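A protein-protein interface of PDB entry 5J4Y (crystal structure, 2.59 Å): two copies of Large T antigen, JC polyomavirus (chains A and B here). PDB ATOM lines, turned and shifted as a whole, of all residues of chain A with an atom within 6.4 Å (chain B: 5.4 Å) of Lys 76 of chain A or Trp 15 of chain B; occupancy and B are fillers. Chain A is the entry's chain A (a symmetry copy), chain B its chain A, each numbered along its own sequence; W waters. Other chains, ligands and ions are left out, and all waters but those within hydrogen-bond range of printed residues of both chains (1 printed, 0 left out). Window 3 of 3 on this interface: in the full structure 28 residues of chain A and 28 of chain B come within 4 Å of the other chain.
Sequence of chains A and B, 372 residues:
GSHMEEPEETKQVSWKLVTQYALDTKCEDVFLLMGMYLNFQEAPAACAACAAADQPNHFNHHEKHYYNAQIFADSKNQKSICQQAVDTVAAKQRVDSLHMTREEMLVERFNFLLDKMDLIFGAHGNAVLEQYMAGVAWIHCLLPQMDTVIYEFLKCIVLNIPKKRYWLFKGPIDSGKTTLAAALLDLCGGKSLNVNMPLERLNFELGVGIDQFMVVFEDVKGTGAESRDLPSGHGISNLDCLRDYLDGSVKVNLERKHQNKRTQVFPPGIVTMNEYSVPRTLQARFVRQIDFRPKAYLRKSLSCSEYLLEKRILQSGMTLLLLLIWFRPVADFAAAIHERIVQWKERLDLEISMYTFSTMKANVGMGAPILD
The side-chain hydroxyl of Thr 19 of chain B sits at hydrogen-bond distance from the backbone carbonyl oxygen of Trp 15 of chain B (3.1 Å). The backbone carbonyl oxygen (O) of Phe 72 of chain A lies within hydrogen-bond range of the side-chain amide nitrogen (NE2) of Gln 78 of chain A. The backbone NH (N) of Asn 77 of chain A lies within hydrogen-bond range of the side-chain hydroxyl (OG) of Ser 75 of chain A, 3.2 Å away.
Position printed for both chains: 77. Of the 8 pairs that touch across the chains among the printed residues, none has its exchanged pair printed and touching as well.
Water W1 lies within hydrogen-bond range of the side-chain amide oxygen of Gln 84 of chain B and the backbone NH of Gln 78 of chain A.
Of chain B, only Gln 12, Trp 15 and Gln 84 come within 4 Å of Lys 76 of chain A. Of chain A, only Lys 76 comes within 4 Å of Trp 15 of chain B. Of the printed residues of chain B, Gln 78 of chain A touches Gln 84 (3.2 Å). Printed residues of chain B within 4 Å of Asn 77 of chain A: Gln 84. Printed residues of chain A within 4 Å of Gln 12 of chain B: Lys 76 (3.9 Å). Leu 17 of chain B touches none of the printed residues of chain A. Val 18 of chain B touches none of the printed residues of chain A. The nearest residue of chain A that does not touch Trp 15 of chain B is Ser 75 of chain A (4.6 Å). The nearest printed residue of chain B that does not touch Ala 73 of chain A is Trp 15 of chain B (5.8 Å).
Among the printed residues, merely in contact across the chains: Ala 73 of chain A with Lys 16 of chain B (3.6 Å), Lys 76 of chain A with Gln 12 of chain B (3.9 Å), Lys 76 of chain A with Trp 15 of chain B (3.4 Å) and Lys 76 of chain A with Gln 84 of chain B (3.5 Å).
Of the 14 printed residues of chain B, 4 touch a printed residue of chain A. Printed residues of chain B that touch a printed residue of chain A: Gln 12, Trp 15, Lys 16 and Gln 84. Hydrophobic or aromatic side chains of chain B within 4 Å of the printed part of chain A: Trp 15. Printed residues of chain A that touch a printed residue of chain B: Ala 73, Asp 74, Ser 75, Lys 76, Asn 77 and Gln 78. Among the printed residues, 8 pairs touch across the chains.
The side-chain amino group (NZ) of Lys 16 of chain B lies within salt-bridge range of the side-chain carboxylate (OD1) of Asp 74 of chain A (3.6 Å). O of Ser 75 of chain A sits at hydrogen-bond distance from NE2 of Gln 84 of chain B, 2.8 Å away. The backbone NH (N) of Asn 77 of chain A lies within hydrogen-bond range of the side-chain amide oxygen (OE1) of Gln 84 of chain B (3.5 Å). The side-chain amide oxygen of Gln 84 of chain B is in hydrogen-bond range of the backbone NH of Gln 78 of chain A.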
ATOM      1  N   PHE A  72     -18.143   5.233 -21.398  1.00  0.00           N
ATOM      2  CA  PHE A  72     -19.127   4.481 -20.630  1.00  0.00           C
ATOM      3  C   PHE A  72     -20.570   4.804 -21.102  1.00  0.00           C
ATOM      4  O   PHE A  72     -21.350   3.879 -21.311  1.00  0.00           O
ATOM      5  CB  PHE A  72     -18.940   4.750 -19.119  1.00  0.00           C
ATOM      6  CG  PHE A  72     -19.824   3.950 -18.193  1.00  0.00           C
ATOM      7  CD1 PHE A  72     -20.985   4.508 -17.659  1.00  0.00           C
ATOM      8  CD2 PHE A  72     -19.484   2.652 -17.834  1.00  0.00           C
ATOM      9  CE1 PHE A  72     -21.810   3.762 -16.804  1.00  0.00           C
ATOM     10  CE2 PHE A  72     -20.298   1.911 -16.970  1.00  0.00           C
ATOM     11  CZ  PHE A  72     -21.444   2.480 -16.445  1.00  0.00           C
ATOM     12  N   ALA A  73     -20.889   6.097 -21.360  1.00  0.00           N
ATOM     13  CA  ALA A  73     -22.211   6.514 -21.851  1.00  0.00           C
ATOM     14  C   ALA A  73     -22.598   5.843 -23.189  1.00  0.00           C
ATOM     15  O   ALA A  73     -23.791   5.809 -23.528  1.00  0.00           O
ATOM     16  CB  ALA A  73     -22.272   8.025 -21.985  1.00  0.00           C
ATOM     17  N   ASP A  74     -21.585   5.302 -23.926  1.00  0.00           N
ATOM     18  CA  ASP A  74     -21.707   4.614 -25.225  1.00  0.00           C
ATOM     19  C   ASP A  74     -21.627   3.087 -25.130  1.00  0.00           C
ATOM     20  O   ASP A  74     -21.816   2.414 -26.145  1.00  0.00           O
ATOM     21  CB  ASP A  74     -20.660   5.135 -26.212  1.00  0.00           C
ATOM     22  CG  ASP A  74     -21.049   6.448 -26.867  1.00  0.00           C
ATOM     23  OD1 ASP A  74     -22.176   6.534 -27.399  1.00  0.00           O
ATOM     24  OD2 ASP A  74     -20.216   7.381 -26.867  1.00  0.00           O
ATOM     25  N   SER A  75     -21.374   2.540 -23.915  1.00  0.00           N
ATOM     26  CA  SER A  75     -21.303   1.107 -23.684  1.00  0.00           C
ATOM     27  C   SER A  75     -22.671   0.396 -23.805  1.00  0.00           C
ATOM     28  O   SER A  75     -23.715   0.940 -23.454  1.00  0.00           O
ATOM     29  CB  SER A  75     -20.661   0.812 -22.336  1.00  0.00           C
ATOM     30  OG  SER A  75     -20.384  -0.575 -22.226  1.00  0.00           O
ATOM     31  N   LYS A  76     -22.626  -0.838 -24.315  1.00  0.00           N
ATOM     32  CA  LYS A  76     -23.751  -1.745 -24.501  1.00  0.00           C
ATOM     33  C   LYS A  76     -23.735  -2.767 -23.358  1.00  0.00           C
ATOM     34  O   LYS A  76     -24.472  -3.749 -23.382  1.00  0.00           O
ATOM     35  CB  LYS A  76     -23.591  -2.490 -25.836  1.00  0.00           C
ATOM     36  CG  LYS A  76     -23.726  -1.618 -27.076  1.00  0.00           C
ATOM     37  CD  LYS A  76     -23.587  -2.475 -28.329  1.00  0.00           C
ATOM     38  CE  LYS A  76     -22.681  -1.834 -29.348  1.00  0.00           C
ATOM     39  NZ  LYS A  76     -22.297  -2.794 -30.417  1.00  0.00           N
ATOM     40  N   ASN A  77     -22.892  -2.527 -22.363  1.00  0.00           N
ATOM     41  CA  ASN A  77     -22.615  -3.443 -21.266  1.00  0.00           C
ATOM     42  C   ASN A  77     -22.257  -2.725 -19.942  1.00  0.00           C
ATOM     43  O   ASN A  77     -21.366  -3.183 -19.243  1.00  0.00           O
ATOM     44  CB  ASN A  77     -21.467  -4.381 -21.712  1.00  0.00           C
ATOM     45  CG  ASN A  77     -21.348  -5.642 -20.903  1.00  0.00           C
ATOM     46  OD1 ASN A  77     -20.247  -6.101 -20.603  1.00  0.00           O
ATOM     47  ND2 ASN A  77     -22.477  -6.219 -20.502  1.00  0.00           N
ATOM     48  N   GLN A  78     -22.992  -1.647 -19.588  1.00  0.00           N
ATOM     49  CA  GLN A  78     -22.833  -0.819 -18.374  1.00  0.00           C
ATOM     50  C   GLN A  78     -22.990  -1.578 -17.045  1.00  0.00           C
ATOM     51  O   GLN A  78     -22.164  -1.384 -16.138  1.00  0.00           O
ATOM     52  CB  GLN A  78     -23.783   0.391 -18.394  1.00  0.00           C
ATOM     53  CG  GLN A  78     -23.648   1.204 -19.677  1.00  0.00           C
ATOM     54  CD  GLN A  78     -24.415   2.481 -19.695  1.00  0.00           C
ATOM     55  OE1 GLN A  78     -25.529   2.588 -19.173  1.00  0.00           O
ATOM     56  NE2 GLN A  78     -23.846   3.484 -20.324  1.00  0.00           N
ATOM     57  N   GLN B  12     -26.051   0.157 -36.770  1.00  0.00           N
ATOM     58  CA  GLN B  12     -26.039  -0.013 -35.314  1.00  0.00           C
ATOM     59  C   GLN B  12     -26.914   1.004 -34.589  1.00  0.00           C
ATOM     60  O   GLN B  12     -26.804   2.206 -34.837  1.00  0.00           O
ATOM     61  CB  GLN B  12     -24.588  -0.013 -34.770  1.00  0.00           C
ATOM     62  CG  GLN B  12     -24.440  -0.462 -33.309  1.00  0.00           C
ATOM     63  CD  GLN B  12     -25.085  -1.792 -33.009  1.00  0.00           C
ATOM     64  OE1 GLN B  12     -24.845  -2.801 -33.687  1.00  0.00           O
ATOM     65  NE2 GLN B  12     -25.931  -1.819 -31.982  1.00  0.00           N
ATOM     66  N   VAL B  13     -27.770   0.507 -33.682  1.00  0.00           N
ATOM     67  CA  VAL B  13     -28.688   1.321 -32.887  1.00  0.00           C
ATOM     68  C   VAL B  13     -27.947   1.975 -31.735  1.00  0.00           C
ATOM     69  O   VAL B  13     -27.091   1.351 -31.110  1.00  0.00           O
ATOM     70  CB  VAL B  13     -30.012   0.586 -32.451  1.00  0.00           C
ATOM     71  CG1 VAL B  13     -29.834  -0.913 -32.333  1.00  0.00           C
ATOM     72  CG2 VAL B  13     -30.647   1.170 -31.193  1.00  0.00           C
ATOM     73  N   SER B  14     -28.255   3.261 -31.493  1.00  0.00           N
ATOM     74  CA  SER B  14     -27.716   4.028 -30.386  1.00  0.00           C
ATOM     75  C   SER B  14     -28.513   3.687 -29.123  1.00  0.00           C
ATOM     76  O   SER B  14     -29.670   4.094 -28.934  1.00  0.00           O
ATOM     77  CB  SER B  14     -27.776   5.519 -30.680  1.00  0.00           C
ATOM     78  OG  SER B  14     -27.478   6.257 -29.504  1.00  0.00           O
ATOM     79  N   TRP B  15     -27.887   2.909 -28.270  1.00  0.00           N
ATOM     80  CA  TRP B  15     -28.411   2.522 -26.976  1.00  0.00           C
ATOM     81  C   TRP B  15     -28.596   3.788 -26.145  1.00  0.00           C
ATOM     82  O   TRP B  15     -29.550   3.885 -25.398  1.00  0.00           O
ATOM     83  CB  TRP B  15     -27.394   1.604 -26.302  1.00  0.00           C
ATOM     84  CG  TRP B  15     -27.328   0.220 -26.867  1.00  0.00           C
ATOM     85  CD1 TRP B  15     -27.118  -0.130 -28.169  1.00  0.00           C
ATOM     86  CD2 TRP B  15     -27.344  -1.006 -26.117  1.00  0.00           C
ATOM     87  NE1 TRP B  15     -27.053  -1.497 -28.288  1.00  0.00           N
ATOM     88  CE2 TRP B  15     -27.197  -2.064 -27.044  1.00  0.00           C
ATOM     89  CE3 TRP B  15     -27.498  -1.319 -24.745  1.00  0.00           C
ATOM     90  CZ2 TRP B  15     -27.186  -3.418 -26.646  1.00  0.00           C
ATOM     91  CZ3 TRP B  15     -27.512  -2.658 -24.355  1.00  0.00           C
ATOM     92  CH2 TRP B  15     -27.346  -3.688 -25.296  1.00  0.00           C
ATOM     93  N   LYS B  16     -27.688   4.755 -26.312  1.00  0.00           N
ATOM     94  CA  LYS B  16     -27.628   6.064 -25.632  1.00  0.00           C
ATOM     95  C   LYS B  16     -28.874   6.877 -25.959  1.00  0.00           C
ATOM     96  O   LYS B  16     -29.436   7.488 -25.050  1.00  0.00           O
ATOM     97  CB  LYS B  16     -26.320   6.799 -26.021  1.00  0.00           C
ATOM     98  CG  LYS B  16     -26.080   8.135 -25.328  1.00  0.00           C
ATOM     99  CD  LYS B  16     -24.635   8.672 -25.487  1.00  0.00           C
ATOM    100  CE  LYS B  16     -24.271   9.091 -26.901  1.00  0.00           C
ATOM    101  NZ  LYS B  16     -23.078   9.987 -26.944  1.00  0.00           N
ATOM    102  N   LEU B  17     -29.336   6.838 -27.239  1.00  0.00           N
ATOM    103  CA  LEU B  17     -30.557   7.520 -27.645  1.00  0.00           C
ATOM    104  C   LEU B  17     -31.817   6.860 -27.038  1.00  0.00           C
ATOM    105  O   LEU B  17     -32.721   7.578 -26.628  1.00  0.00           O
ATOM    106  CB  LEU B  17     -30.675   7.619 -29.176  1.00  0.00           C
ATOM    107  CG  LEU B  17     -30.641   9.024 -29.878  1.00  0.00           C
ATOM    108  CD1 LEU B  17     -31.475   8.998 -31.130  1.00  0.00           C
ATOM    109  CD2 LEU B  17     -31.156  10.188 -28.984  1.00  0.00           C
ATOM    110  N   VAL B  18     -31.889   5.519 -26.966  1.00  0.00           N
ATOM    111  CA  VAL B  18     -33.036   4.844 -26.342  1.00  0.00           C
ATOM    112  C   VAL B  18     -33.105   5.198 -24.824  1.00  0.00           C
ATOM    113  O   VAL B  18     -34.195   5.409 -24.269  1.00  0.00           O
ATOM    114  CB  VAL B  18     -33.041   3.310 -26.590  1.00  0.00           C
ATOM    115  CG1 VAL B  18     -34.276   2.648 -25.971  1.00  0.00           C
ATOM    116  CG2 VAL B  18     -32.962   2.992 -28.082  1.00  0.00           C
ATOM    117  N   THR B  19     -31.926   5.275 -24.174  1.00  0.00           N
ATOM    118  CA  THR B  19     -31.779   5.618 -22.765  1.00  0.00           C
ATOM    119  C   THR B  19     -32.250   7.055 -22.547  1.00  0.00           C
ATOM    120  O   THR B  19     -32.915   7.338 -21.557  1.00  0.00           O
ATOM    121  CB  THR B  19     -30.328   5.355 -22.340  1.00  0.00           C
ATOM    122  OG1 THR B  19     -30.096   3.942 -22.332  1.00  0.00           O
ATOM    123  CG2 THR B  19     -29.978   5.958 -20.995  1.00  0.00           C
ATOM    124  N   GLN B  20     -31.925   7.947 -23.479  1.00  0.00           N
ATOM    125  CA  GLN B  20     -32.295   9.343 -23.394  1.00  0.00           C
ATOM    126  C   GLN B  20     -33.806   9.479 -23.410  1.00  0.00           C
ATOM    127  O   GLN B  20     -34.349  10.232 -22.593  1.00  0.00           O
ATOM    128  CB  GLN B  20     -31.624  10.155 -24.521  1.00  0.00           C
ATOM    129  CG  GLN B  20     -31.398  11.635 -24.173  1.00  0.00           C
ATOM    130  CD  GLN B  20     -30.630  11.847 -22.878  1.00  0.00           C
ATOM    131  OE1 GLN B  20     -29.439  11.506 -22.759  1.00  0.00           O
ATOM    132  NE2 GLN B  20     -31.307  12.403 -21.873  1.00  0.00           N
ATOM    133  N   ASN B  68     -33.238   6.007 -35.588  1.00  0.00           N
ATOM    134  CA  ASN B  68     -32.794   5.015 -34.606  1.00  0.00           C
ATOM    135  C   ASN B  68     -33.866   3.943 -34.407  1.00  0.00           C
ATOM    136  O   ASN B  68     -33.516   2.781 -34.233  1.00  0.00           O
ATOM    137  CB  ASN B  68     -32.399   5.671 -33.260  1.00  0.00           C
ATOM    138  CG  ASN B  68     -31.512   4.813 -32.392  1.00  0.00           C
ATOM    139  OD1 ASN B  68     -30.491   4.261 -32.841  1.00  0.00           O
ATOM    140  ND2 ASN B  68     -31.875   4.697 -31.122  1.00  0.00           N
ATOM    141  N   ASN B  77     -31.666  -7.886 -30.599  1.00  0.00           N
ATOM    142  CA  ASN B  77     -31.375  -7.681 -29.188  1.00  0.00           C
ATOM    143  C   ASN B  77     -32.114  -6.465 -28.578  1.00  0.00           C
ATOM    144  O   ASN B  77     -31.519  -5.746 -27.790  1.00  0.00           O
ATOM    145  CB  ASN B  77     -29.840  -7.525 -29.040  1.00  0.00           C
ATOM    146  CG  ASN B  77     -29.328  -7.742 -27.643  1.00  0.00           C
ATOM    147  OD1 ASN B  77     -28.426  -7.043 -27.184  1.00  0.00           O
ATOM    148  ND2 ASN B  77     -29.910  -8.694 -26.921  1.00  0.00           N
ATOM    149  N   SER B  80     -32.581  -6.260 -24.390  1.00  0.00           N
ATOM    150  CA  SER B  80     -31.340  -5.869 -23.695  1.00  0.00           C
ATOM    151  C   SER B  80     -31.140  -4.369 -23.755  1.00  0.00           C
ATOM    152  O   SER B  80     -30.726  -3.763 -22.758  1.00  0.00           O
ATOM    153  CB  SER B  80     -30.124  -6.538 -24.318  1.00  0.00           C
ATOM    154  OG  SER B  80     -30.280  -7.937 -24.276  1.00  0.00           O
ATOM    155  N   ILE B  81     -31.397  -3.782 -24.934  1.00  0.00           N
ATOM    156  CA  ILE B  81     -31.300  -2.346 -25.173  1.00  0.00           C
ATOM    157  C   ILE B  81     -32.222  -1.616 -24.210  1.00  0.00           C
ATOM    158  O   ILE B  81     -31.790  -0.694 -23.539  1.00  0.00           O
ATOM    159  CB  ILE B  81     -31.572  -2.002 -26.675  1.00  0.00           C
ATOM    160  CG1 ILE B  81     -30.614  -2.808 -27.600  1.00  0.00           C
ATOM    161  CG2 ILE B  81     -31.444  -0.485 -26.920  1.00  0.00           C
ATOM    162  CD1 ILE B  81     -30.721  -2.572 -29.092  1.00  0.00           C
ATOM    163  N   GLN B  84     -31.035  -1.888 -20.255  1.00  0.00           N
ATOM    164  CA  GLN B  84     -30.041  -0.897 -19.863  1.00  0.00           C
ATOM    165  C   GLN B  84     -30.665   0.491 -19.742  1.00  0.00           C
ATOM    166  O   GLN B  84     -30.287   1.238 -18.832  1.00  0.00           O
ATOM    167  CB  GLN B  84     -28.878  -0.891 -20.848  1.00  0.00           C
ATOM    168  CG  GLN B  84     -27.778   0.119 -20.537  1.00  0.00           C
ATOM    169  CD  GLN B  84     -26.558  -0.207 -21.336  1.00  0.00           C
ATOM    170  OE1 GLN B  84     -25.845  -1.189 -21.069  1.00  0.00           O
ATOM    171  NE2 GLN B  84     -26.313   0.596 -22.350  1.00  0.00           N
HETATM  172  O   HOH W   1     -26.088  -3.065 -18.983  1.00  0.00           O
